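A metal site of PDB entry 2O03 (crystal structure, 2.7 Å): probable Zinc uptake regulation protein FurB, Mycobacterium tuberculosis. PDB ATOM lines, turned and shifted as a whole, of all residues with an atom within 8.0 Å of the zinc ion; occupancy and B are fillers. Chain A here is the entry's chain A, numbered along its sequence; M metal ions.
N of Asp 62 lies within hydrogen-bond range of O of Arg 74. A ring nitrogen (ND1) of His 81 lies within hydrogen-bond range of the backbone carbonyl oxygen (O) of His 79, 2.9 Å away. The backbone NH of Cys 76 sits at hydrogen-bond distance from the backbone carbonyl oxygen of Leu 60 (3.3 Å).
The side-chain carboxylate (OD2) of Asp 62 binds the zinc ion (2.0 Å). NE2 of His 83 binds the zinc ion (2.0 Å). The zinc ion is bound by a ring nitrogen (NE2) of His 81, at 2.1 Å. SG of Cys 76 is bound to the zinc ion (2.3 Å).
Four residues have an atom within 4 Å of the zinc ion: Asp 62, Cys 76, His 81 and His 83. The nearest printed residue that does not touch the zinc ion is Ser 77 (4.3 Å).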
ATOM      1  N   PHE A  26      29.900 -21.320  14.449  1.00  0.00           N
ATOM      2  CA  PHE A  26      28.660 -20.690  13.965  1.00  0.00           C
ATOM      3  C   PHE A  26      28.882 -19.548  12.966  1.00  0.00           C
ATOM      4  O   PHE A  26      29.674 -18.647  13.233  1.00  0.00           O
ATOM      5  CB  PHE A  26      27.878 -20.139  15.162  1.00  0.00           C
ATOM      6  CG  PHE A  26      27.087 -21.177  15.883  1.00  0.00           C
ATOM      7  CD1 PHE A  26      25.795 -21.485  15.494  1.00  0.00           C
ATOM      8  CD2 PHE A  26      27.640 -21.859  16.963  1.00  0.00           C
ATOM      9  CE1 PHE A  26      25.065 -22.444  16.172  1.00  0.00           C
ATOM     10  CE2 PHE A  26      26.902 -22.826  17.654  1.00  0.00           C
ATOM     11  CZ  PHE A  26      25.603 -23.113  17.242  1.00  0.00           C
ATOM     12  N   GLY A  59      17.253 -30.969  11.495  1.00  0.00           N
ATOM     13  CA  GLY A  59      18.221 -31.414  12.466  1.00  0.00           C
ATOM     14  C   GLY A  59      19.572 -31.791  11.894  1.00  0.00           C
ATOM     15  O   GLY A  59      20.190 -32.740  12.376  1.00  0.00           O
ATOM     16  N   LEU A  60      20.015 -31.064  10.879  1.00  0.00           N
ATOM     17  CA  LEU A  60      21.340 -31.235  10.328  1.00  0.00           C
ATOM     18  C   LEU A  60      22.246 -30.128  10.815  1.00  0.00           C
ATOM     19  O   LEU A  60      23.391 -30.383  11.154  1.00  0.00           O
ATOM     20  CB  LEU A  60      21.315 -31.290   8.797  1.00  0.00           C
ATOM     21  CG  LEU A  60      20.632 -32.529   8.184  1.00  0.00           C
ATOM     22  CD1 LEU A  60      19.899 -32.163   6.894  1.00  0.00           C
ATOM     23  CD2 LEU A  60      21.626 -33.711   7.969  1.00  0.00           C
ATOM     24  N   VAL A  61      21.742 -28.887  10.855  1.00  0.00           N
ATOM     25  CA  VAL A  61      22.473 -27.791  11.526  1.00  0.00           C
ATOM     26  C   VAL A  61      21.780 -27.305  12.813  1.00  0.00           C
ATOM     27  O   VAL A  61      20.568 -27.405  12.964  1.00  0.00           O
ATOM     28  CB  VAL A  61      22.743 -26.543  10.606  1.00  0.00           C
ATOM     29  CG1 VAL A  61      23.276 -26.929   9.250  1.00  0.00           C
ATOM     30  CG2 VAL A  61      21.503 -25.644  10.496  1.00  0.00           C
ATOM     31  N   ASP A  62      22.582 -26.778  13.725  1.00  0.00           N
ATOM     32  CA  ASP A  62      22.093 -26.122  14.922  1.00  0.00           C
ATOM     33  C   ASP A  62      22.121 -24.604  14.729  1.00  0.00           C
ATOM     34  O   ASP A  62      22.915 -24.101  13.942  1.00  0.00           O
ATOM     35  CB  ASP A  62      22.979 -26.491  16.096  1.00  0.00           C
ATOM     36  CG  ASP A  62      22.844 -27.944  16.467  1.00  0.00           C
ATOM     37  OD1 ASP A  62      22.008 -28.666  15.864  1.00  0.00           O
ATOM     38  OD2 ASP A  62      23.575 -28.370  17.373  1.00  0.00           O
ATOM     39  N   THR A  63      21.292 -23.888  15.460  1.00  0.00           N
ATOM     40  CA  THR A  63      21.147 -22.469  15.232  1.00  0.00           C
ATOM     41  C   THR A  63      21.214 -21.603  16.509  1.00  0.00           C
ATOM     42  O   THR A  63      20.951 -22.098  17.624  1.00  0.00           O
ATOM     43  CB  THR A  63      19.848 -22.214  14.406  1.00  0.00           C
ATOM     44  OG1 THR A  63      20.013 -21.055  13.578  1.00  0.00           O
ATOM     45  CG2 THR A  63      18.639 -22.042  15.296  1.00  0.00           C
ATOM     46  N   ARG A  74      25.669 -24.034  12.301  1.00  0.00           N
ATOM     47  CA  ARG A  74      26.793 -24.995  12.304  1.00  0.00           C
ATOM     48  C   ARG A  74      26.286 -26.433  12.062  1.00  0.00           C
ATOM     49  O   ARG A  74      25.270 -26.833  12.648  1.00  0.00           O
ATOM     50  CB  ARG A  74      27.595 -24.940  13.689  1.00  0.00           C
ATOM     51  N   ARG A  75      27.010 -27.251  11.270  1.00  0.00           N
ATOM     52  CA  ARG A  75      26.748 -28.720  11.259  1.00  0.00           C
ATOM     53  C   ARG A  75      26.878 -29.149  12.694  1.00  0.00           C
ATOM     54  O   ARG A  75      27.741 -28.634  13.378  1.00  0.00           O
ATOM     55  CB  ARG A  75      27.746 -29.505  10.392  1.00  0.00           C
ATOM     56  N   CYS A  76      26.022 -30.076  13.139  1.00  0.00           N
ATOM     57  CA  CYS A  76      25.944 -30.512  14.530  1.00  0.00           C
ATOM     58  C   CYS A  76      27.323 -30.806  15.135  1.00  0.00           C
ATOM     59  O   CYS A  76      28.176 -31.400  14.457  1.00  0.00           O
ATOM     60  CB  CYS A  76      25.022 -31.697  14.680  1.00  0.00           C
ATOM     61  SG  CYS A  76      24.352 -31.802  16.342  1.00  0.00           S
ATOM     62  N   SER A  77      27.508 -30.388  16.393  1.00  0.00           N
ATOM     63  CA  SER A  77      28.845 -29.991  16.958  1.00  0.00           C
ATOM     64  C   SER A  77      29.966 -31.030  17.270  1.00  0.00           C
ATOM     65  O   SER A  77      31.081 -30.616  17.651  1.00  0.00           O
ATOM     66  CB  SER A  77      28.643 -29.047  18.168  1.00  0.00           C
ATOM     67  N   GLU A  78      29.700 -32.337  17.125  1.00  0.00           N
ATOM     68  CA  GLU A  78      30.665 -33.443  17.426  1.00  0.00           C
ATOM     69  C   GLU A  78      30.983 -33.676  18.935  1.00  0.00           C
ATOM     70  O   GLU A  78      31.044 -34.819  19.386  1.00  0.00           O
ATOM     71  CB  GLU A  78      31.951 -33.371  16.567  1.00  0.00           C
ATOM     72  N   HIS A  79      31.163 -32.597  19.699  1.00  0.00           N
ATOM     73  CA  HIS A  79      31.243 -32.671  21.158  1.00  0.00           C
ATOM     74  C   HIS A  79      29.865 -32.919  21.777  1.00  0.00           C
ATOM     75  O   HIS A  79      28.869 -32.345  21.330  1.00  0.00           O
ATOM     76  CB  HIS A  79      31.877 -31.401  21.709  1.00  0.00           C
ATOM     77  CG  HIS A  79      33.317 -31.205  21.303  1.00  0.00           C
ATOM     78  ND1 HIS A  79      34.364 -31.875  21.911  1.00  0.00           N
ATOM     79  CD2 HIS A  79      33.886 -30.429  20.346  1.00  0.00           C
ATOM     80  CE1 HIS A  79      35.509 -31.512  21.356  1.00  0.00           C
ATOM     81  NE2 HIS A  79      35.248 -30.640  20.405  1.00  0.00           N
ATOM     82  N   HIS A  80      29.806 -33.785  22.793  1.00  0.00           N
ATOM     83  CA  HIS A  80      28.513 -34.221  23.387  1.00  0.00           C
ATOM     84  C   HIS A  80      27.666 -33.064  23.940  1.00  0.00           C
ATOM     85  O   HIS A  80      28.113 -32.327  24.813  1.00  0.00           O
ATOM     86  CB  HIS A  80      28.741 -35.322  24.458  1.00  0.00           C
ATOM     87  CG  HIS A  80      27.509 -35.731  25.193  1.00  0.00           C
ATOM     88  ND1 HIS A  80      26.881 -36.941  24.981  1.00  0.00           N
ATOM     89  CD2 HIS A  80      26.810 -35.121  26.193  1.00  0.00           C
ATOM     90  CE1 HIS A  80      25.837 -37.044  25.796  1.00  0.00           C
ATOM     91  NE2 HIS A  80      25.771 -35.963  26.535  1.00  0.00           N
ATOM     92  N   HIS A  81      26.458 -32.925  23.387  1.00  0.00           N
ATOM     93  CA  HIS A  81      25.489 -31.932  23.846  1.00  0.00           C
ATOM     94  C   HIS A  81      24.067 -32.431  23.635  1.00  0.00           C
ATOM     95  O   HIS A  81      23.866 -33.515  23.085  1.00  0.00           O
ATOM     96  CB  HIS A  81      25.700 -30.613  23.127  1.00  0.00           C
ATOM     97  CG  HIS A  81      25.444 -30.692  21.644  1.00  0.00           C
ATOM     98  ND1 HIS A  81      26.440 -30.977  20.735  1.00  0.00           N
ATOM     99  CD2 HIS A  81      24.309 -30.502  20.928  1.00  0.00           C
ATOM    100  CE1 HIS A  81      25.923 -30.977  19.519  1.00  0.00           C
ATOM    101  NE2 HIS A  81      24.635 -30.687  19.602  1.00  0.00           N
ATOM    102  N   HIS A  82      23.074 -31.656  24.076  1.00  0.00           N
ATOM    103  CA  HIS A  82      21.682 -31.951  23.766  1.00  0.00           C
ATOM    104  C   HIS A  82      21.009 -30.759  23.029  1.00  0.00           C
ATOM    105  O   HIS A  82      21.626 -29.698  22.852  1.00  0.00           O
ATOM    106  CB  HIS A  82      20.904 -32.376  25.046  1.00  0.00           C
ATOM    107  CG  HIS A  82      21.569 -33.475  25.829  1.00  0.00           C
ATOM    108  ND1 HIS A  82      21.496 -34.807  25.465  1.00  0.00           N
ATOM    109  CD2 HIS A  82      22.306 -33.437  26.964  1.00  0.00           C
ATOM    110  CE1 HIS A  82      22.177 -35.544  26.333  1.00  0.00           C
ATOM    111  NE2 HIS A  82      22.667 -34.736  27.265  1.00  0.00           N
ATOM    112  N   HIS A  83      19.752 -30.950  22.595  1.00  0.00           N
ATOM    113  CA  HIS A  83      19.040 -29.934  21.838  1.00  0.00           C
ATOM    114  C   HIS A  83      17.725 -29.482  22.419  1.00  0.00           C
ATOM    115  O   HIS A  83      16.966 -30.269  22.975  1.00  0.00           O
ATOM    116  CB  HIS A  83      18.726 -30.423  20.441  1.00  0.00           C
ATOM    117  CG  HIS A  83      19.898 -30.935  19.688  1.00  0.00           C
ATOM    118  ND1 HIS A  83      20.055 -32.257  19.361  1.00  0.00           N
ATOM    119  CD2 HIS A  83      20.974 -30.285  19.172  1.00  0.00           C
ATOM    120  CE1 HIS A  83      21.185 -32.423  18.696  1.00  0.00           C
ATOM    121  NE2 HIS A  83      21.751 -31.237  18.560  1.00  0.00           N
ATOM    122  N   LEU A  84      17.452 -28.190  22.226  1.00  0.00           N
ATOM    123  CA  LEU A  84      16.148 -27.569  22.400  1.00  0.00           C
ATOM    124  C   LEU A  84      15.464 -27.541  21.032  1.00  0.00           C
ATOM    125  O   LEU A  84      16.110 -27.214  20.035  1.00  0.00           O
ATOM    126  CB  LEU A  84      16.381 -26.150  22.871  1.00  0.00           C
ATOM    127  CG  LEU A  84      15.224 -25.177  23.036  1.00  0.00           C
ATOM    128  CD1 LEU A  84      14.158 -25.719  23.994  1.00  0.00           C
ATOM    129  CD2 LEU A  84      15.813 -23.891  23.555  1.00  0.00           C
ATOM    130  N   THR A  92      16.303 -26.094  15.676  1.00  0.00           N
ATOM    131  CA  THR A  92      17.125 -26.808  16.653  1.00  0.00           C
ATOM    132  C   THR A  92      18.225 -25.902  17.243  1.00  0.00           C
ATOM    133  O   THR A  92      19.049 -25.344  16.494  1.00  0.00           O
ATOM    134  CB  THR A  92      17.829 -28.049  16.031  1.00  0.00           C
ATOM    135  OG1 THR A  92      16.983 -28.671  15.059  1.00  0.00           O
ATOM    136  CG2 THR A  92      18.196 -29.035  17.099  1.00  0.00           C
ATOM    137  N   ILE A  93      18.239 -25.790  18.562  1.00  0.00           N
ATOM    138  CA  ILE A  93      19.231 -25.002  19.280  1.00  0.00           C
ATOM    139  C   ILE A  93      20.028 -25.934  20.158  1.00  0.00           C
ATOM    140  O   ILE A  93      19.450 -26.844  20.753  1.00  0.00           O
ATOM    141  CB  ILE A  93      18.557 -23.896  20.110  1.00  0.00           C
ATOM    142  CG1 ILE A  93      17.976 -22.862  19.165  1.00  0.00           C
ATOM    143  CG2 ILE A  93      19.557 -23.227  21.080  1.00  0.00           C
ATOM    144  CD1 ILE A  93      17.200 -21.780  19.819  1.00  0.00           C
ATOM    145  N   GLU A  94      21.348 -25.721  20.212  1.00  0.00           N
ATOM    146  CA  GLU A  94      22.263 -26.525  21.040  1.00  0.00           C
ATOM    147  C   GLU A  94      22.217 -26.092  22.499  1.00  0.00           C
ATOM    148  O   GLU A  94      22.291 -24.886  22.786  1.00  0.00           O
ATOM    149  CB  GLU A  94      23.694 -26.368  20.547  1.00  0.00           C
ATOM    150  CG  GLU A  94      24.723 -27.065  21.437  1.00  0.00           C
ATOM    151  CD  GLU A  94      26.138 -27.021  20.879  1.00  0.00           C
ATOM    152  OE1 GLU A  94      26.322 -26.721  19.673  1.00  0.00           O
ATOM    153  OE2 GLU A  94      27.066 -27.281  21.672  1.00  0.00           O
ATOM    154  N   VAL A  95      22.104 -27.068  23.393  1.00  0.00           N
ATOM    155  CA  VAL A  95      22.110 -26.831  24.856  1.00  0.00           C
ATOM    156  C   VAL A  95      22.957 -27.862  25.613  1.00  0.00           C
ATOM    157  O   VAL A  95      23.129 -28.991  25.154  1.00  0.00           O
ATOM    158  CB  VAL A  95      20.658 -26.771  25.492  1.00  0.00           C
ATOM    159  CG1 VAL A  95      19.870 -25.562  24.977  1.00  0.00           C
ATOM    160  CG2 VAL A  95      19.873 -28.070  25.254  1.00  0.00           C
HETATM  161 ZN    ZN M   1      23.434 -30.303  17.888  1.00  0.00          ZN
